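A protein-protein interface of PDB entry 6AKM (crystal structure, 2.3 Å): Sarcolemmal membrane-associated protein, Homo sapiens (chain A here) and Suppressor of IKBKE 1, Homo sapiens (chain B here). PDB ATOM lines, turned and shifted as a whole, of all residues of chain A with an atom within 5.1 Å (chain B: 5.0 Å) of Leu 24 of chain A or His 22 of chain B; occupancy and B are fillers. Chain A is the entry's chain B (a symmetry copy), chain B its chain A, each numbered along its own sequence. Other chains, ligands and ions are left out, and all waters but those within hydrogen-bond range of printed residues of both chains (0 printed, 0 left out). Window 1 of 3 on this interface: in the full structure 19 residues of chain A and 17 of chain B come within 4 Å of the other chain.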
ATOM      1  N   GLU A  17      19.139 -15.216  11.260  1.00  0.00           N
ATOM      2  CA  GLU A  17      20.034 -14.146  11.663  1.00  0.00           C
ATOM      3  C   GLU A  17      20.946 -14.602  12.802  1.00  0.00           C
ATOM      4  O   GLU A  17      22.072 -14.116  12.928  1.00  0.00           O
ATOM      5  CB  GLU A  17      19.228 -12.901  12.052  1.00  0.00           C
ATOM      6  CG  GLU A  17      20.063 -11.648  12.050  1.00  0.00           C
ATOM      7  CD  GLU A  17      20.894 -11.462  13.315  1.00  0.00           C
ATOM      8  OE1 GLU A  17      20.605 -12.115  14.351  1.00  0.00           O
ATOM      9  OE2 GLU A  17      21.911 -10.735  13.220  1.00  0.00           O
ATOM     10  N   LEU A  20      23.676 -16.328  10.875  1.00  0.00           N
ATOM     11  CA  LEU A  20      24.613 -15.341  10.370  1.00  0.00           C
ATOM     12  C   LEU A  20      25.573 -14.885  11.463  1.00  0.00           C
ATOM     13  O   LEU A  20      26.785 -14.826  11.236  1.00  0.00           O
ATOM     14  CB  LEU A  20      23.856 -14.149   9.792  1.00  0.00           C
ATOM     15  CG  LEU A  20      24.583 -13.365   8.697  1.00  0.00           C
ATOM     16  CD1 LEU A  20      23.611 -12.434   7.985  1.00  0.00           C
ATOM     17  CD2 LEU A  20      25.808 -12.613   9.177  1.00  0.00           C
ATOM     18  N   GLU A  21      25.053 -14.579  12.659  1.00  0.00           N
ATOM     19  CA  GLU A  21      25.922 -14.109  13.737  1.00  0.00           C
ATOM     20  C   GLU A  21      26.955 -15.168  14.117  1.00  0.00           C
ATOM     21  O   GLU A  21      28.115 -14.844  14.390  1.00  0.00           O
ATOM     22  CB  GLU A  21      25.104 -13.719  14.968  1.00  0.00           C
ATOM     23  CG  GLU A  21      25.979 -13.222  16.133  1.00  0.00           C
ATOM     24  CD  GLU A  21      26.433 -14.336  17.083  1.00  0.00           C
ATOM     25  OE1 GLU A  21      27.287 -14.068  17.960  1.00  0.00           O
ATOM     26  OE2 GLU A  21      25.937 -15.478  16.955  1.00  0.00           O
ATOM     27  N   GLN A  22      26.562 -16.406  14.104  1.00  0.00           N
ATOM     28  CA  GLN A  22      27.491 -17.494  14.423  1.00  0.00           C
ATOM     29  C   GLN A  22      28.594 -17.485  13.371  1.00  0.00           C
ATOM     30  O   GLN A  22      29.665 -17.706  13.733  1.00  0.00           O
ATOM     31  CB  GLN A  22      26.805 -18.849  14.493  1.00  0.00           C
ATOM     32  CG  GLN A  22      26.816 -19.462  15.873  1.00  0.00           C
ATOM     33  CD  GLN A  22      26.755 -20.973  15.880  1.00  0.00           C
ATOM     34  OE1 GLN A  22      27.392 -21.648  16.684  1.00  0.00           O
ATOM     35  NE2 GLN A  22      25.992 -21.524  14.964  1.00  0.00           N
ATOM     36  N   LYS A  23      28.305 -17.202  12.144  1.00  0.00           N
ATOM     37  CA  LYS A  23      29.382 -17.105  11.165  1.00  0.00           C
ATOM     38  C   LYS A  23      30.248 -15.884  11.428  1.00  0.00           C
ATOM     39  O   LYS A  23      31.481 -15.963  11.325  1.00  0.00           O
ATOM     40  CB  LYS A  23      28.823 -17.103   9.746  1.00  0.00           C
ATOM     41  CG  LYS A  23      28.091 -18.404   9.372  1.00  0.00           C
ATOM     42  CD  LYS A  23      27.592 -18.349   7.934  1.00  0.00           C
ATOM     43  CE  LYS A  23      26.857 -19.627   7.524  1.00  0.00           C
ATOM     44  NZ  LYS A  23      25.680 -19.872   8.392  1.00  0.00           N
ATOM     45  N   LEU A  24      29.640 -14.753  11.804  1.00  0.00           N
ATOM     46  CA  LEU A  24      30.454 -13.568  12.081  1.00  0.00           C
ATOM     47  C   LEU A  24      31.377 -13.810  13.264  1.00  0.00           C
ATOM     48  O   LEU A  24      32.536 -13.373  13.259  1.00  0.00           O
ATOM     49  CB  LEU A  24      29.575 -12.353  12.355  1.00  0.00           C
ATOM     50  CG  LEU A  24      28.630 -11.920  11.233  1.00  0.00           C
ATOM     51  CD1 LEU A  24      27.789 -10.720  11.657  1.00  0.00           C
ATOM     52  CD2 LEU A  24      29.408 -11.622   9.964  1.00  0.00           C
ATOM     53  N   ALA A  25      30.880 -14.513  14.289  1.00  0.00           N
ATOM     54  CA  ALA A  25      31.725 -14.817  15.439  1.00  0.00           C
ATOM     55  C   ALA A  25      32.879 -15.736  15.037  1.00  0.00           C
ATOM     56  O   ALA A  25      34.004 -15.578  15.514  1.00  0.00           O
ATOM     57  CB  ALA A  25      30.886 -15.444  16.556  1.00  0.00           C
ATOM     58  N   THR A  26      32.628 -16.687  14.144  1.00  0.00           N
ATOM     59  CA  THR A  26      33.717 -17.528  13.659  1.00  0.00           C
ATOM     60  C   THR A  26      34.725 -16.701  12.877  1.00  0.00           C
ATOM     61  O   THR A  26      35.937 -16.893  13.005  1.00  0.00           O
ATOM     62  CB  THR A  26      33.160 -18.636  12.783  1.00  0.00           C
ATOM     63  OG1 THR A  26      32.082 -19.295  13.472  1.00  0.00           O
ATOM     64  CG2 THR A  26      34.264 -19.625  12.423  1.00  0.00           C
ATOM     65  N   LEU A  27      34.236 -15.768  12.072  1.00  0.00           N
ATOM     66  CA  LEU A  27      35.132 -14.865  11.363  1.00  0.00           C
ATOM     67  C   LEU A  27      36.019 -14.096  12.323  1.00  0.00           C
ATOM     68  O   LEU A  27      37.231 -14.001  12.114  1.00  0.00           O
ATOM     69  CB  LEU A  27      34.327 -13.898  10.510  1.00  0.00           C
ATOM     70  CG  LEU A  27      34.227 -14.381   9.084  1.00  0.00           C
ATOM     71  CD1 LEU A  27      33.030 -13.700   8.444  1.00  0.00           C
ATOM     72  CD2 LEU A  27      35.524 -14.105   8.321  1.00  0.00           C
ATOM     73  N   GLN A  28      35.426 -13.520  13.377  1.00  0.00           N
ATOM     74  CA  GLN A  28      36.219 -12.721  14.307  1.00  0.00           C
ATOM     75  C   GLN A  28      37.378 -13.533  14.864  1.00  0.00           C
ATOM     76  O   GLN A  28      38.511 -13.047  14.928  1.00  0.00           O
ATOM     77  CB  GLN A  28      35.344 -12.193  15.447  1.00  0.00           C
ATOM     78  CG  GLN A  28      36.052 -11.196  16.337  1.00  0.00           C
ATOM     79  CD  GLN A  28      36.965 -11.843  17.367  1.00  0.00           C
ATOM     80  OE1 GLN A  28      36.615 -12.854  17.977  1.00  0.00           O
ATOM     81  NE2 GLN A  28      38.141 -11.258  17.569  1.00  0.00           N
ATOM     82  N   ARG B  18      18.872  -7.050  16.953  1.00  0.00           N
ATOM     83  CA  ARG B  18      19.999  -7.938  16.702  1.00  0.00           C
ATOM     84  C   ARG B  18      20.717  -7.547  15.427  1.00  0.00           C
ATOM     85  O   ARG B  18      21.943  -7.642  15.354  1.00  0.00           O
ATOM     86  CB  ARG B  18      19.550  -9.398  16.631  1.00  0.00           C
ATOM     87  CG  ARG B  18      19.240  -9.973  17.978  1.00  0.00           C
ATOM     88  CD  ARG B  18      18.619 -11.328  17.842  1.00  0.00           C
ATOM     89  NE  ARG B  18      18.186 -11.845  19.135  1.00  0.00           N
ATOM     90  CZ  ARG B  18      17.678 -13.058  19.309  1.00  0.00           C
ATOM     91  NH1 ARG B  18      17.540 -13.864  18.265  1.00  0.00           N
ATOM     92  NH2 ARG B  18      17.308 -13.464  20.517  1.00  0.00           N
ATOM     93  N   LEU B  19      19.973  -7.094  14.413  1.00  0.00           N
ATOM     94  CA  LEU B  19      20.623  -6.637  13.192  1.00  0.00           C
ATOM     95  C   LEU B  19      21.523  -5.444  13.478  1.00  0.00           C
ATOM     96  O   LEU B  19      22.614  -5.331  12.915  1.00  0.00           O
ATOM     97  CB  LEU B  19      19.585  -6.281  12.126  1.00  0.00           C
ATOM     98  CG  LEU B  19      18.982  -7.444  11.332  1.00  0.00           C
ATOM     99  CD1 LEU B  19      17.733  -6.990  10.564  1.00  0.00           C
ATOM    100  CD2 LEU B  19      19.989  -8.055  10.380  1.00  0.00           C
ATOM    101  N   ARG B  20      21.101  -4.563  14.377  1.00  0.00           N
ATOM    102  CA  ARG B  20      21.922  -3.400  14.688  1.00  0.00           C
ATOM    103  C   ARG B  20      23.224  -3.806  15.366  1.00  0.00           C
ATOM    104  O   ARG B  20      24.306  -3.358  14.965  1.00  0.00           O
ATOM    105  CB  ARG B  20      21.133  -2.421  15.545  1.00  0.00           C
ATOM    106  CG  ARG B  20      20.119  -1.644  14.713  1.00  0.00           C
ATOM    107  CD  ARG B  20      19.334  -0.639  15.526  1.00  0.00           C
ATOM    108  NE  ARG B  20      18.563   0.250  14.655  1.00  0.00           N
ATOM    109  CZ  ARG B  20      17.511   0.968  15.050  1.00  0.00           C
ATOM    110  NH1 ARG B  20      16.874   1.748  14.185  1.00  0.00           N
ATOM    111  NH2 ARG B  20      17.087   0.897  16.307  1.00  0.00           N
ATOM    112  N   GLU B  21      23.152  -4.666  16.390  1.00  0.00           N
ATOM    113  CA  GLU B  21      24.384  -5.016  17.083  1.00  0.00           C
ATOM    114  C   GLU B  21      25.267  -5.903  16.217  1.00  0.00           C
ATOM    115  O   GLU B  21      26.488  -5.925  16.393  1.00  0.00           O
ATOM    116  CB  GLU B  21      24.087  -5.685  18.426  1.00  0.00           C
ATOM    117  CG  GLU B  21      23.323  -6.971  18.349  1.00  0.00           C
ATOM    118  CD  GLU B  21      22.975  -7.503  19.727  1.00  0.00           C
ATOM    119  OE1 GLU B  21      23.723  -8.366  20.235  1.00  0.00           O
ATOM    120  OE2 GLU B  21      21.964  -7.052  20.309  1.00  0.00           O
ATOM    121  N   HIS B  22      24.682  -6.622  15.264  1.00  0.00           N
ATOM    122  CA  HIS B  22      25.525  -7.450  14.422  1.00  0.00           C
ATOM    123  C   HIS B  22      26.070  -6.662  13.242  1.00  0.00           C
ATOM    124  O   HIS B  22      27.139  -6.999  12.717  1.00  0.00           O
ATOM    125  CB  HIS B  22      24.761  -8.698  13.984  1.00  0.00           C
ATOM    126  CG  HIS B  22      24.301  -9.534  15.139  1.00  0.00           C
ATOM    127  ND1 HIS B  22      23.124 -10.255  15.125  1.00  0.00           N
ATOM    128  CD2 HIS B  22      24.853  -9.742  16.359  1.00  0.00           C
ATOM    129  CE1 HIS B  22      22.971 -10.870  16.286  1.00  0.00           C
ATOM    130  NE2 HIS B  22      24.005 -10.574  17.054  1.00  0.00           N
ATOM    131  N   ASP B  23      25.367  -5.609  12.826  1.00  0.00           N
ATOM    132  CA  ASP B  23      25.943  -4.682  11.865  1.00  0.00           C
ATOM    133  C   ASP B  23      27.138  -3.955  12.466  1.00  0.00           C
ATOM    134  O   ASP B  23      28.138  -3.720  11.778  1.00  0.00           O
ATOM    135  CB  ASP B  23      24.866  -3.722  11.352  1.00  0.00           C
ATOM    136  CG  ASP B  23      25.434  -2.566  10.526  1.00  0.00           C
ATOM    137  OD1 ASP B  23      25.847  -2.822   9.372  1.00  0.00           O
ATOM    138  OD2 ASP B  23      25.555  -1.435  11.059  1.00  0.00           O
ATOM    139  N   ALA B  24      27.084  -3.643  13.760  1.00  0.00           N
ATOM    140  CA  ALA B  24      28.282  -3.141  14.426  1.00  0.00           C
ATOM    141  C   ALA B  24      29.376  -4.199  14.458  1.00  0.00           C
ATOM    142  O   ALA B  24      30.551  -3.895  14.223  1.00  0.00           O
ATOM    143  CB  ALA B  24      27.949  -2.676  15.841  1.00  0.00           C
ATOM    144  N   ALA B  25      29.018  -5.449  14.755  1.00  0.00           N
ATOM    145  CA  ALA B  25      30.027  -6.504  14.767  1.00  0.00           C
ATOM    146  C   ALA B  25      30.720  -6.612  13.416  1.00  0.00           C
ATOM    147  O   ALA B  25      31.935  -6.828  13.345  1.00  0.00           O
ATOM    148  CB  ALA B  25      29.389  -7.839  15.149  1.00  0.00           C
ATOM    149  N   ALA B  26      29.962  -6.474  12.330  1.00  0.00           N
ATOM    150  CA  ALA B  26      30.579  -6.530  11.014  1.00  0.00           C
ATOM    151  C   ALA B  26      31.507  -5.347  10.807  1.00  0.00           C
ATOM    152  O   ALA B  26      32.533  -5.470  10.130  1.00  0.00           O
ATOM    153  CB  ALA B  26      29.502  -6.566   9.926  1.00  0.00           C
ATOM    154  N   LEU B  29      34.679  -6.190  12.314  1.00  0.00           N
ATOM    155  CA  LEU B  29      35.364  -7.142  11.450  1.00  0.00           C
ATOM    156  C   LEU B  29      36.083  -6.438  10.316  1.00  0.00           C
ATOM    157  O   LEU B  29      37.198  -6.833   9.945  1.00  0.00           O
ATOM    158  CB  LEU B  29      34.398  -8.173  10.871  1.00  0.00           C
ATOM    159  CG  LEU B  29      33.712  -9.162  11.804  1.00  0.00           C
ATOM    160  CD1 LEU B  29      32.659  -9.931  11.001  1.00  0.00           C
ATOM    161  CD2 LEU B  29      34.747 -10.131  12.328  1.00  0.00           C
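O of Arg 18 of chain B sits at hydrogen-bond distance from ND1 of His 22 of chain B, 2.9 Å away.
Of the 10 printed residues of chain B, 4 touch a printed residue of chain A.
Hydrophobic or aromatic side chains of chain A that line the printed part of chain B: Leu 24.
Among the printed residues, 7 pairs touch across the chains.
Printed residues of chain B within 4 Å of Leu 24 of chain A: His 22 (3.9 Å) and Leu 29 (3.8 Å).
Printed residues of chain A within 4 Å of Arg 18 of chain B: Glu 17 (3.7 Å).
Of the printed residues of chain B, Gln 28 of chain A touches Leu 29 (3.6 Å).
Printed residues of chain B within 4 Å of Glu 21 of chain A: His 22.
Of the printed residues of chain A, Leu 19 of chain B touches Glu 17.
Of the printed residues of chain A, Leu 29 of chain B touches Leu 24 (3.8 Å) and Gln 28 (3.6 Å).
Lys 23 of chain A touches none of the printed residues of chain B.
Asp 23 of chain B touches none of the printed residues of chain A.
The nearest printed residue of chain A that does not touch His 22 of chain B is Leu 20 of chain A (6.3 Å).
The nearest printed residue of chain B that does not touch Glu 21 of chain A is Ala 25 of chain B (6.4 Å).
ND1 of His 22 of chain B lies close to OE1 of Glu 17 of chain A, 3.2 Å away.
Among the printed residues, pairs that only touch across the chains: Glu 17 of chain A with Arg 18 of chain B, Glu 17 of chain A with Leu 19 of chain B, Glu 21 of chain A with His 22 of chain B, Leu 24 of chain A with His 22 of chain B, Leu 24 of chain A with Leu 29 of chain B and Gln 28 of chain A with Leu 29 of chain B.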
